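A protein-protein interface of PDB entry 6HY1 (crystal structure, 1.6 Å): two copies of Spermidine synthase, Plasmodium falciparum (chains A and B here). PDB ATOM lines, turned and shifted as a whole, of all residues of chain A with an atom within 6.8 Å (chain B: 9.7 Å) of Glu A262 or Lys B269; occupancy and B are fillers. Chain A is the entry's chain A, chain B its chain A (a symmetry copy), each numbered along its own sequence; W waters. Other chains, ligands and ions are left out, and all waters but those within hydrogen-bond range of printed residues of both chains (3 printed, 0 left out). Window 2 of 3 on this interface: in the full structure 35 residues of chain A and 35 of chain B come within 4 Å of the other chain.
Glu A262 touches Lys B269, and with the chains exchanged Lys A269 touches Glu B262. Asn A263 touches Lys B269, and with the chains exchanged Lys A269 touches Asn B263. Ala A266 touches its own counterpart, Ala B266. Ala A266 touches Lys B269, and with the chains exchanged Lys A269 touches Ala B266. Positions printed for both chains: 262, 263, 264, 265, 266, 267 and 269. Of the 14 pairs that touch across the chains among the printed residues, 7 have their exchanged pair printed and touching as well.
The side-chain amide oxygen (OD1) of Asn B263 lies close to the backbone carbonyl oxygen (O) of Lys A269 (3.2 Å). The backbone carbonyl oxygen (O) of Tyr A258 lies within hydrogen-bond range of the backbone NH (N) of Ala B272 (3.0 Å). O of Leu B270 lies within hydrogen-bond range of ND2 of Asn A263 (2.9 Å). The backbone carbonyl oxygen (O) of Lys B269 sits close to the side-chain amide oxygen (OD1) of Asn A263, at 3.2 Å.
Water W2 lies within hydrogen-bond range of the side-chain amide oxygen of Asn A263, the backbone carbonyl oxygen of Leu B270 and the side-chain amide nitrogen of Asn A260. Water W1 lies within hydrogen-bond range of the backbone carbonyl oxygen of Lys A269 and the side-chain amide oxygen of Asn B263. Water W3 lies within hydrogen-bond range of the backbone carbonyl oxygen (O) of Lys B269 (2.8 Å) and the side-chain amide oxygen (OD1) of Asn A263 (3.4 Å).
Of the 24 printed residues of chain B, 8 touch a printed residue of chain A. Printed residues of chain B that touch a printed residue of chain A: Glu B262, Asn B263, Ala B266, Lys B269, Leu B270, Pro B271, Ala B272 and Leu B275. Printed residues of chain A that touch a printed residue of chain B: Tyr A258, Tyr A259, Asn A260, Glu A262, Asn A263, Ala A266 and Lys A269. Among the printed residues, no Asp or Glu carboxylate lies within 4 Å of a Lys or Arg side-chain nitrogen of the other chain.
The side-chain amide oxygen (OD1) of Asn A260 sits close to the backbone NH (N) of Glu A262 (3.3 Å). ND2 of Asn A263 is in hydrogen-bond range of O of Tyr A258, at 2.8 Å. The side-chain hydroxyl (OH) of Tyr A259 sits at hydrogen-bond distance from a ring nitrogen (ND1) of His A264. The backbone NH (N) of Asn A263 lies within hydrogen-bond range of the side-chain amide oxygen (OD1) of Asn A260, 2.8 Å away.
Tyr A258 touches Pro B271 (O to CA, 3.7 Å). Tyr A259 touches Ala B272. Asn A260 touches Leu B270. Asn A260 touches Leu B275. OE1 of Glu A262 touches CD of Lys B269, at 3.5 Å. Pro B271 touches Asn A263. CB of Ala A266 touches O of Ala B266, at 3.997 Å. Ala A266 touches Lys B269. OE1 of Glu B262 touches CD of Lys A269, 3.5 Å away. CB of Lys A269 touches CB of Ala B266 (3.6 Å).
Printed residues of chain B within 4 Å of Tyr A258: Pro B271 (3.7 Å) and Ala B272 (3.0 Å). Of the printed residues of chain B, Tyr A259 touches Ala B272. Asn A260 touches just these residues of chain B: Leu B270 (3.7 Å) and Leu B275 (3.6 Å). Of chain B, only Lys B269 (3.5 Å) comes within 4 Å of Glu A262. Printed residues of chain B within 4 Å of Lys A269: Glu B262 (3.5 Å), Asn B263 (3.2 Å) and Ala B266 (3.6 Å). Printed residues of chain A within 4 Å of Ala B266: Ala A266 and Lys A269. Of chain A, only Glu A262, Asn A263 and Ala A266 come within 4 Å of Lys B269. Of the printed residues of chain A, Leu B275 touches Asn A260 (3.6 Å).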
ATOM      1  N   PRO A 244      13.732  15.643  18.128  1.00  0.00           N
ATOM      2  CA  PRO A 244      13.052  14.635  17.308  1.00  0.00           C
ATOM      3  C   PRO A 244      13.683  14.540  15.928  1.00  0.00           C
ATOM      4  O   PRO A 244      14.240  15.514  15.420  1.00  0.00           O
ATOM      5  CB  PRO A 244      11.614  15.162  17.198  1.00  0.00           C
ATOM      6  CG  PRO A 244      11.731  16.631  17.471  1.00  0.00           C
ATOM      7  CD  PRO A 244      12.843  16.770  18.447  1.00  0.00           C
ATOM      8  N   TYR A 258      -1.124  17.240  23.419  1.00  0.00           N
ATOM      9  CA  TYR A 258      -0.042  17.861  24.166  1.00  0.00           C
ATOM     10  C   TYR A 258       1.231  17.917  23.329  1.00  0.00           C
ATOM     11  O   TYR A 258       1.761  19.004  23.049  1.00  0.00           O
ATOM     12  CB  TYR A 258       0.220  17.093  25.468  1.00  0.00           C
ATOM     13  CG  TYR A 258       1.173  17.781  26.471  1.00  0.00           C
ATOM     14  CD1 TYR A 258       2.537  17.719  26.308  1.00  0.00           C
ATOM     15  CD2 TYR A 258       0.672  18.413  27.628  1.00  0.00           C
ATOM     16  CE1 TYR A 258       3.419  18.316  27.227  1.00  0.00           C
ATOM     17  CE2 TYR A 258       1.537  19.020  28.553  1.00  0.00           C
ATOM     18  CZ  TYR A 258       2.917  18.963  28.342  1.00  0.00           C
ATOM     19  OH  TYR A 258       3.809  19.543  29.245  1.00  0.00           O
ATOM     20  N   TYR A 259       1.752  16.748  22.952  1.00  0.00           N
ATOM     21  CA  TYR A 259       3.008  16.672  22.210  1.00  0.00           C
ATOM     22  C   TYR A 259       2.969  17.468  20.907  1.00  0.00           C
ATOM     23  O   TYR A 259       1.994  17.401  20.138  1.00  0.00           O
ATOM     24  CB  TYR A 259       3.350  15.207  21.870  1.00  0.00           C
ATOM     25  CG  TYR A 259       4.675  15.081  21.167  1.00  0.00           C
ATOM     26  CD1 TYR A 259       4.752  15.157  19.761  1.00  0.00           C
ATOM     27  CD2 TYR A 259       5.854  14.859  21.879  1.00  0.00           C
ATOM     28  CE1 TYR A 259       5.955  15.066  19.115  1.00  0.00           C
ATOM     29  CE2 TYR A 259       7.076  14.762  21.218  1.00  0.00           C
ATOM     30  CZ  TYR A 259       7.113  14.840  19.842  1.00  0.00           C
ATOM     31  OH  TYR A 259       8.336  14.755  19.192  1.00  0.00           O
ATOM     32  N   ASN A 260       4.052  18.207  20.658  1.00  0.00           N
ATOM     33  CA  ASN A 260       4.406  18.619  19.300  1.00  0.00           C
ATOM     34  C   ASN A 260       5.919  18.759  19.187  1.00  0.00           C
ATOM     35  O   ASN A 260       6.683  18.571  20.144  1.00  0.00           O
ATOM     36  CB  ASN A 260       3.638  19.882  18.866  1.00  0.00           C
ATOM     37  CG  ASN A 260       3.974  21.131  19.733  1.00  0.00           C
ATOM     38  OD1 ASN A 260       5.085  21.283  20.247  1.00  0.00           O
ATOM     39  ND2 ASN A 260       2.963  21.970  19.942  1.00  0.00           N
ATOM     40  N   TYR A 261       6.374  19.057  17.955  1.00  0.00           N
ATOM     41  CA  TYR A 261       7.798  19.053  17.659  1.00  0.00           C
ATOM     42  C   TYR A 261       8.561  20.052  18.526  1.00  0.00           C
ATOM     43  O   TYR A 261       9.663  19.764  19.013  1.00  0.00           O
ATOM     44  CB  TYR A 261       7.960  19.352  16.164  1.00  0.00           C
ATOM     45  CG  TYR A 261       9.370  19.356  15.640  1.00  0.00           C
ATOM     46  CD1 TYR A 261      10.190  20.464  15.810  1.00  0.00           C
ATOM     47  CD2 TYR A 261       9.870  18.271  14.939  1.00  0.00           C
ATOM     48  CE1 TYR A 261      11.500  20.486  15.313  1.00  0.00           C
ATOM     49  CE2 TYR A 261      11.175  18.284  14.426  1.00  0.00           C
ATOM     50  CZ  TYR A 261      11.979  19.389  14.624  1.00  0.00           C
ATOM     51  OH  TYR A 261      13.264  19.386  14.130  1.00  0.00           O
ATOM     52  N   GLU A 262       7.978  21.220  18.762  1.00  0.00           N
ATOM     53  CA  GLU A 262       8.670  22.206  19.604  1.00  0.00           C
ATOM     54  C   GLU A 262       8.656  21.850  21.107  1.00  0.00           C
ATOM     55  O   GLU A 262       9.674  22.040  21.794  1.00  0.00           O
ATOM     56  CB  GLU A 262       8.045  23.580  19.342  1.00  0.00           C
ATOM     57  CG  GLU A 262       8.393  24.093  17.919  1.00  0.00           C
ATOM     58  CD  GLU A 262       8.116  25.581  17.723  1.00  0.00           C
ATOM     59  OE1 GLU A 262       7.248  26.142  18.438  1.00  0.00           O
ATOM     60  OE2 GLU A 262       8.778  26.192  16.849  1.00  0.00           O
ATOM     61  N   ASN A 263       7.541  21.286  21.616  1.00  0.00           N
ATOM     62  CA  ASN A 263       7.446  20.899  23.032  1.00  0.00           C
ATOM     63  C   ASN A 263       8.446  19.843  23.386  1.00  0.00           C
ATOM     64  O   ASN A 263       8.876  19.743  24.541  1.00  0.00           O
ATOM     65  CB  ASN A 263       6.065  20.337  23.338  1.00  0.00           C
ATOM     66  CG  ASN A 263       5.062  21.369  23.235  1.00  0.00           C
ATOM     67  OD1 ASN A 263       5.424  22.558  23.210  1.00  0.00           O
ATOM     68  ND2 ASN A 263       3.801  20.983  23.140  1.00  0.00           N
ATOM     69  N   HIS A 264       8.719  18.960  22.428  1.00  0.00           N
ATOM     70  CA  HIS A 264       9.652  17.886  22.667  1.00  0.00           C
ATOM     71  C   HIS A 264      10.941  18.442  23.239  1.00  0.00           C
ATOM     72  O   HIS A 264      11.415  18.015  24.294  1.00  0.00           O
ATOM     73  CB  HIS A 264       9.834  17.141  21.325  1.00  0.00           C
ATOM     74  CG  HIS A 264      10.807  16.011  21.367  1.00  0.00           C
ATOM     75  ND1 HIS A 264      10.622  14.854  20.627  1.00  0.00           N
ATOM     76  CD2 HIS A 264      11.970  15.855  22.035  1.00  0.00           C
ATOM     77  CE1 HIS A 264      11.645  14.043  20.846  1.00  0.00           C
ATOM     78  NE2 HIS A 264      12.476  14.625  21.691  1.00  0.00           N
ATOM     79  N   SER A 265      11.552  19.406  22.526  1.00  0.00           N
ATOM     80  CA  SER A 265      12.831  19.942  22.978  1.00  0.00           C
ATOM     81  C   SER A 265      12.665  20.836  24.194  1.00  0.00           C
ATOM     82  O   SER A 265      13.527  20.844  25.074  1.00  0.00           O
ATOM     83  CB  SER A 265      13.496  20.734  21.838  1.00  0.00           C
ATOM     84  OG  SER A 265      13.229  20.071  20.601  1.00  0.00           O
ATOM     85  N   ALA A 266      11.539  21.552  24.273  1.00  0.00           N
ATOM     86  CA  ALA A 266      11.335  22.494  25.375  1.00  0.00           C
ATOM     87  C   ALA A 266      11.261  21.785  26.724  1.00  0.00           C
ATOM     88  O   ALA A 266      11.623  22.359  27.774  1.00  0.00           O
ATOM     89  CB  ALA A 266      10.055  23.290  25.121  1.00  0.00           C
ATOM     90  N   ALA A 267      10.783  20.533  26.721  1.00  0.00           N
ATOM     91  CA  ALA A 267      10.603  19.782  27.951  1.00  0.00           C
ATOM     92  C   ALA A 267      11.919  19.532  28.655  1.00  0.00           C
ATOM     93  O   ALA A 267      11.924  19.250  29.855  1.00  0.00           O
ATOM     94  CB  ALA A 267       9.883  18.449  27.634  1.00  0.00           C
ATOM     95  N   LYS A 269      14.386  21.793  28.950  1.00  0.00           N
ATOM     96  CA  LYS A 269      14.928  23.068  29.445  1.00  0.00           C
ATOM     97  C   LYS A 269      14.470  23.257  30.892  1.00  0.00           C
ATOM     98  O   LYS A 269      13.350  23.699  31.145  1.00  0.00           O
ATOM     99  CB  LYS A 269      14.473  24.201  28.535  1.00  0.00           C
ATOM    100  CG  LYS A 269      14.920  24.027  27.067  1.00  0.00           C
ATOM    101  CD  LYS A 269      16.423  23.777  27.017  1.00  0.00           C
ATOM    102  CE  LYS A 269      16.975  23.739  25.577  1.00  0.00           C
ATOM    103  NZ  LYS A 269      16.101  24.492  24.629  1.00  0.00           N
ATOM    104  N   MET B  65      10.332  34.350  36.805  1.00  0.00           N
ATOM    105  CA  MET B  65       9.899  34.310  35.413  1.00  0.00           C
ATOM    106  C   MET B  65       9.108  35.557  35.054  1.00  0.00           C
ATOM    107  O   MET B  65       9.307  36.130  33.978  1.00  0.00           O
ATOM    108  CB  MET B  65       9.088  33.029  35.115  1.00  0.00           C
ATOM    109  CG  MET B  65       9.923  31.755  35.248  1.00  0.00           C
ATOM    110  SD  MET B  65      11.244  31.682  33.966  1.00  0.00           S
ATOM    111  CE  MET B  65      10.185  31.650  32.539  1.00  0.00           C
ATOM    112  N   LEU B 193      -3.445  26.969  32.179  1.00  0.00           N
ATOM    113  CA  LEU B 193      -3.959  26.382  30.942  1.00  0.00           C
ATOM    114  C   LEU B 193      -4.722  25.092  31.197  1.00  0.00           C
ATOM    115  O   LEU B 193      -5.440  24.619  30.298  1.00  0.00           O
ATOM    116  CB  LEU B 193      -2.814  26.129  29.963  1.00  0.00           C
ATOM    117  CG  LEU B 193      -1.641  25.245  30.377  1.00  0.00           C
ATOM    118  CD1 LEU B 193      -1.958  23.752  30.123  1.00  0.00           C
ATOM    119  CD2 LEU B 193      -0.337  25.677  29.649  1.00  0.00           C
ATOM    120  N   GLU B 215       1.663  37.147  23.507  1.00  0.00           N
ATOM    121  CA  GLU B 215       2.159  35.784  23.655  1.00  0.00           C
ATOM    122  C   GLU B 215       1.806  35.277  25.054  1.00  0.00           C
ATOM    123  O   GLU B 215       1.529  36.057  25.967  1.00  0.00           O
ATOM    124  CB  GLU B 215       3.657  35.704  23.415  1.00  0.00           C
ATOM    125  CG  GLU B 215       4.033  36.203  22.003  1.00  0.00           C
ATOM    126  CD  GLU B 215       5.447  36.731  21.875  1.00  0.00           C
ATOM    127  OE1 GLU B 215       5.916  37.495  22.749  1.00  0.00           O
ATOM    128  OE2 GLU B 215       6.115  36.385  20.876  1.00  0.00           O
ATOM    129  N   TYR B 216       1.779  33.953  25.207  1.00  0.00           N
ATOM    130  CA  TYR B 216       1.394  33.311  26.464  1.00  0.00           C
ATOM    131  C   TYR B 216       2.506  32.335  26.830  1.00  0.00           C
ATOM    132  O   TYR B 216       2.946  31.535  25.997  1.00  0.00           O
ATOM    133  CB  TYR B 216       0.036  32.624  26.330  1.00  0.00           C
ATOM    134  CG  TYR B 216      -0.461  31.966  27.595  1.00  0.00           C
ATOM    135  CD1 TYR B 216      -0.031  30.682  27.957  1.00  0.00           C
ATOM    136  CD2 TYR B 216      -1.380  32.615  28.401  1.00  0.00           C
ATOM    137  CE1 TYR B 216      -0.503  30.080  29.141  1.00  0.00           C
ATOM    138  CE2 TYR B 216      -1.857  32.013  29.571  1.00  0.00           C
ATOM    139  CZ  TYR B 216      -1.413  30.745  29.919  1.00  0.00           C
ATOM    140  OH  TYR B 216      -1.893  30.160  31.076  1.00  0.00           O
ATOM    141  N   ALA B 217       2.994  32.429  28.049  1.00  0.00           N
ATOM    142  CA  ALA B 217       4.043  31.559  28.552  1.00  0.00           C
ATOM    143  C   ALA B 217       3.493  30.799  29.755  1.00  0.00           C
ATOM    144  O   ALA B 217       2.505  31.219  30.359  1.00  0.00           O
ATOM    145  CB  ALA B 217       5.297  32.342  28.935  1.00  0.00           C
ATOM    146  N   ASN B 218       4.156  29.690  30.119  1.00  0.00           N
ATOM    147  CA  ASN B 218       3.742  28.870  31.260  1.00  0.00           C
ATOM    148  C   ASN B 218       4.870  28.719  32.273  1.00  0.00           C
ATOM    149  O   ASN B 218       6.048  28.627  31.898  1.00  0.00           O
ATOM    150  CB  ASN B 218       3.281  27.480  30.786  1.00  0.00           C
ATOM    151  CG  ASN B 218       2.591  26.714  31.889  1.00  0.00           C
ATOM    152  OD1 ASN B 218       1.683  27.237  32.538  1.00  0.00           O
ATOM    153  ND2 ASN B 218       3.027  25.484  32.117  1.00  0.00           N
ATOM    154  N   ILE B 219       4.516  28.754  33.568  1.00  0.00           N
ATOM    155  CA  ILE B 219       5.453  28.628  34.684  1.00  0.00           C
ATOM    156  C   ILE B 219       5.038  27.414  35.513  1.00  0.00           C
ATOM    157  O   ILE B 219       3.873  27.290  35.872  1.00  0.00           O
ATOM    158  CB  ILE B 219       5.448  29.872  35.612  1.00  0.00           C
ATOM    159  CG1 ILE B 219       5.639  31.165  34.807  1.00  0.00           C
ATOM    160  CG2 ILE B 219       6.551  29.727  36.674  1.00  0.00           C
ATOM    161  CD1 ILE B 219       5.483  32.423  35.686  1.00  0.00           C
ATOM    162  N   THR B 242       9.528  36.476  23.426  1.00  0.00           N
ATOM    163  CA  THR B 242      10.010  35.095  23.545  1.00  0.00           C
ATOM    164  C   THR B 242      11.528  34.963  23.606  1.00  0.00           C
ATOM    165  O   THR B 242      12.021  33.937  24.087  1.00  0.00           O
ATOM    166  CB  THR B 242       9.471  34.213  22.412  1.00  0.00           C
ATOM    167  OG1 THR B 242      10.074  34.590  21.159  1.00  0.00           O
ATOM    168  CG2 THR B 242       7.959  34.351  22.306  1.00  0.00           C
ATOM    169  N   LYS B 243      12.297  35.954  23.146  1.00  0.00           N
ATOM    170  CA  LYS B 243      13.743  35.792  23.066  1.00  0.00           C
ATOM    171  C   LYS B 243      14.453  36.867  23.878  1.00  0.00           C
ATOM    172  O   LYS B 243      14.304  38.060  23.558  1.00  0.00           O
ATOM    173  CB  LYS B 243      14.212  35.841  21.590  1.00  0.00           C
ATOM    174  CG  LYS B 243      13.432  34.904  20.634  1.00  0.00           C
ATOM    175  CD  LYS B 243      13.400  33.416  21.082  1.00  0.00           C
ATOM    176  CE  LYS B 243      12.591  32.522  20.096  1.00  0.00           C
ATOM    177  NZ  LYS B 243      12.098  31.222  20.684  1.00  0.00           N
ATOM    178  N   GLU B 262      17.854  29.796  28.471  1.00  0.00           N
ATOM    179  CA  GLU B 262      17.110  28.792  27.700  1.00  0.00           C
ATOM    180  C   GLU B 262      15.648  28.615  28.168  1.00  0.00           C
ATOM    181  O   GLU B 262      14.746  28.466  27.327  1.00  0.00           O
ATOM    182  CB  GLU B 262      17.887  27.473  27.758  1.00  0.00           C
ATOM    183  CG  GLU B 262      19.208  27.563  26.949  1.00  0.00           C
ATOM    184  CD  GLU B 262      19.844  26.205  26.666  1.00  0.00           C
ATOM    185  OE1 GLU B 262      19.600  25.241  27.437  1.00  0.00           O
ATOM    186  OE2 GLU B 262      20.588  26.101  25.661  1.00  0.00           O
ATOM    187  N   ASN B 263      15.393  28.683  29.491  1.00  0.00           N
ATOM    188  CA  ASN B 263      14.029  28.543  30.024  1.00  0.00           C
ATOM    189  C   ASN B 263      13.129  29.635  29.538  1.00  0.00           C
ATOM    190  O   ASN B 263      11.910  29.450  29.436  1.00  0.00           O
ATOM    191  CB  ASN B 263      14.043  28.611  31.545  1.00  0.00           C
ATOM    192  CG  ASN B 263      14.708  27.457  32.099  1.00  0.00           C
ATOM    193  OD1 ASN B 263      14.912  26.473  31.368  1.00  0.00           O
ATOM    194  ND2 ASN B 263      15.096  27.527  33.361  1.00  0.00           N
ATOM    195  N   HIS B 264      13.702  30.823  29.364  1.00  0.00           N
ATOM    196  CA  HIS B 264      12.924  31.954  28.919  1.00  0.00           C
ATOM    197  C   HIS B 264      12.132  31.577  27.682  1.00  0.00           C
ATOM    198  O   HIS B 264      10.910  31.735  27.626  1.00  0.00           O
ATOM    199  CB  HIS B 264      13.911  33.121  28.697  1.00  0.00           C
ATOM    200  CG  HIS B 264      13.287  34.378  28.189  1.00  0.00           C
ATOM    201  ND1 HIS B 264      13.737  35.630  28.575  1.00  0.00           N
ATOM    202  CD2 HIS B 264      12.270  34.586  27.325  1.00  0.00           C
ATOM    203  CE1 HIS B 264      13.013  36.550  27.955  1.00  0.00           C
ATOM    204  NE2 HIS B 264      12.122  35.945  27.191  1.00  0.00           N
ATOM    205  N   SER B 265      12.832  31.087  26.642  1.00  0.00           N
ATOM    206  CA  SER B 265      12.149  30.767  25.395  1.00  0.00           C
ATOM    207  C   SER B 265      11.308  29.508  25.524  1.00  0.00           C
ATOM    208  O   SER B 265      10.232  29.423  24.929  1.00  0.00           O
ATOM    209  CB  SER B 265      13.181  30.588  24.266  1.00  0.00           C
ATOM    210  OG  SER B 265      14.234  31.535  24.452  1.00  0.00           O
ATOM    211  N   ALA B 266      11.767  28.552  26.336  1.00  0.00           N
ATOM    212  CA  ALA B 266      11.054  27.278  26.459  1.00  0.00           C
ATOM    213  C   ALA B 266       9.665  27.459  27.064  1.00  0.00           C
ATOM    214  O   ALA B 266       8.732  26.678  26.779  1.00  0.00           O
ATOM    215  CB  ALA B 266      11.887  26.321  27.311  1.00  0.00           C
ATOM    216  N   ALA B 267       9.509  28.482  27.917  1.00  0.00           N
ATOM    217  CA  ALA B 267       8.252  28.713  28.606  1.00  0.00           C
ATOM    218  C   ALA B 267       7.131  29.034  27.641  1.00  0.00           C
ATOM    219  O   ALA B 267       5.960  28.894  28.000  1.00  0.00           O
ATOM    220  CB  ALA B 267       8.438  29.854  29.637  1.00  0.00           C
ATOM    221  N   PHE B 268       7.470  29.426  26.396  1.00  0.00           N
ATOM    222  CA  PHE B 268       6.480  29.819  25.412  1.00  0.00           C
ATOM    223  C   PHE B 268       6.078  28.665  24.486  1.00  0.00           C
ATOM    224  O   PHE B 268       5.209  28.847  23.629  1.00  0.00           O
ATOM    225  CB  PHE B 268       6.993  30.982  24.559  1.00  0.00           C
ATOM    226  CG  PHE B 268       7.055  32.308  25.324  1.00  0.00           C
ATOM    227  CD1 PHE B 268       8.135  32.610  26.101  1.00  0.00           C
ATOM    228  CD2 PHE B 268       6.012  33.206  25.228  1.00  0.00           C
ATOM    229  CE1 PHE B 268       8.209  33.846  26.815  1.00  0.00           C
ATOM    230  CE2 PHE B 268       6.070  34.440  25.955  1.00  0.00           C
ATOM    231  CZ  PHE B 268       7.174  34.742  26.701  1.00  0.00           C
ATOM    232  N   LYS B 269       6.646  27.489  24.698  1.00  0.00           N
ATOM    233  CA  LYS B 269       6.337  26.299  23.891  1.00  0.00           C
ATOM    234  C   LYS B 269       5.202  25.534  24.573  1.00  0.00           C
ATOM    235  O   LYS B 269       5.432  24.770  25.510  1.00  0.00           O
ATOM    236  CB  LYS B 269       7.595  25.455  23.728  1.00  0.00           C
ATOM    237  CG  LYS B 269       8.757  26.211  23.046  1.00  0.00           C
ATOM    238  CD  LYS B 269       8.269  26.828  21.740  1.00  0.00           C
ATOM    239  CE  LYS B 269       9.405  27.476  20.924  1.00  0.00           C
ATOM    240  NZ  LYS B 269      10.736  26.887  21.261  1.00  0.00           N
ATOM    241  N   LEU B 270       3.989  25.760  24.113  1.00  0.00           N
ATOM    242  CA  LEU B 270       2.764  25.405  24.808  1.00  0.00           C
ATOM    243  C   LEU B 270       2.245  24.058  24.331  1.00  0.00           C
ATOM    244  O   LEU B 270       2.556  23.619  23.222  1.00  0.00           O
ATOM    245  CB  LEU B 270       1.698  26.473  24.559  1.00  0.00           C
ATOM    246  CG  LEU B 270       2.132  27.900  24.983  1.00  0.00           C
ATOM    247  CD1 LEU B 270       1.010  28.843  24.573  1.00  0.00           C
ATOM    248  CD2 LEU B 270       2.370  27.892  26.458  1.00  0.00           C
ATOM    249  N   PRO B 271       1.441  23.383  25.147  1.00  0.00           N
ATOM    250  CA  PRO B 271       0.806  22.131  24.689  1.00  0.00           C
ATOM    251  C   PRO B 271      -0.106  22.336  23.488  1.00  0.00           C
ATOM    252  O   PRO B 271      -0.787  23.356  23.348  1.00  0.00           O
ATOM    253  CB  PRO B 271      -0.002  21.671  25.915  1.00  0.00           C
ATOM    254  CG  PRO B 271       0.622  22.359  27.107  1.00  0.00           C
ATOM    255  CD  PRO B 271       1.302  23.605  26.601  1.00  0.00           C
ATOM    256  N   ALA B 272      -0.210  21.280  22.659  1.00  0.00           N
ATOM    257  CA  ALA B 272      -0.955  21.379  21.399  1.00  0.00           C
ATOM    258  C   ALA B 272      -2.383  21.873  21.584  1.00  0.00           C
ATOM    259  O   ALA B 272      -2.877  22.663  20.773  1.00  0.00           O
ATOM    260  CB  ALA B 272      -0.955  20.016  20.696  1.00  0.00           C
ATOM    261  N   PHE B 273      -3.109  21.358  22.588  1.00  0.00           N
ATOM    262  CA  PHE B 273      -4.521  21.702  22.681  1.00  0.00           C
ATOM    263  C   PHE B 273      -4.722  23.194  22.932  1.00  0.00           C
ATOM    264  O   PHE B 273      -5.752  23.756  22.532  1.00  0.00           O
ATOM    265  CB  PHE B 273      -5.206  20.883  23.788  1.00  0.00           C
ATOM    266  CG  PHE B 273      -4.979  21.412  25.193  1.00  0.00           C
ATOM    267  CD1 PHE B 273      -5.778  22.426  25.689  1.00  0.00           C
ATOM    268  CD2 PHE B 273      -3.992  20.875  26.012  1.00  0.00           C
ATOM    269  CE1 PHE B 273      -5.590  22.918  26.980  1.00  0.00           C
ATOM    270  CE2 PHE B 273      -3.792  21.358  27.318  1.00  0.00           C
ATOM    271  CZ  PHE B 273      -4.599  22.377  27.806  1.00  0.00           C
ATOM    272  N   LEU B 274      -3.778  23.833  23.629  1.00  0.00           N
ATOM    273  CA  LEU B 274      -3.914  25.261  23.924  1.00  0.00           C
ATOM    274  C   LEU B 274      -3.660  26.101  22.670  1.00  0.00           C
ATOM    275  O   LEU B 274      -4.437  27.010  22.344  1.00  0.00           O
ATOM    276  CB  LEU B 274      -2.949  25.650  25.053  1.00  0.00           C
ATOM    277  CG  LEU B 274      -2.920  27.151  25.401  1.00  0.00           C
ATOM    278  CD1 LEU B 274      -4.288  27.608  25.870  1.00  0.00           C
ATOM    279  CD2 LEU B 274      -1.857  27.450  26.444  1.00  0.00           C
ATOM    280  N   LEU B 275      -2.579  25.795  21.951  1.00  0.00           N
ATOM    281  CA  LEU B 275      -2.339  26.431  20.652  1.00  0.00           C
ATOM    282  C   LEU B 275      -3.585  26.397  19.785  1.00  0.00           C
ATOM    283  O   LEU B 275      -3.952  27.398  19.151  1.00  0.00           O
ATOM    284  CB  LEU B 275      -1.192  25.732  19.941  1.00  0.00           C
ATOM    285  CG  LEU B 275       0.155  25.867  20.634  1.00  0.00           C
ATOM    286  CD1 LEU B 275       1.214  25.107  19.894  1.00  0.00           C
ATOM    287  CD2 LEU B 275       0.528  27.354  20.723  1.00  0.00           C
ATOM    288  N   ILE B 278      -6.415  29.025  20.898  1.00  0.00           N
ATOM    289  CA  ILE B 278      -6.203  30.459  20.776  1.00  0.00           C
ATOM    290  C   ILE B 278      -5.974  30.867  19.333  1.00  0.00           C
ATOM    291  O   ILE B 278      -5.728  32.041  19.060  1.00  0.00           O
ATOM    292  CB  ILE B 278      -5.045  30.939  21.668  1.00  0.00           C
ATOM    293  CG1 ILE B 278      -3.719  30.338  21.219  1.00  0.00           C
ATOM    294  CG2 ILE B 278      -5.319  30.639  23.146  1.00  0.00           C
ATOM    295  CD1 ILE B 278      -2.621  30.527  22.227  1.00  0.00           C
HETATM  296  O   HOH W   1      12.018  25.424  32.841  1.00  0.00           O
HETATM  297  O   HOH W   2       4.644  24.168  21.370  1.00  0.00           O
HETATM  298  O   HOH W   3       4.723  22.308  26.541  1.00  0.00           O
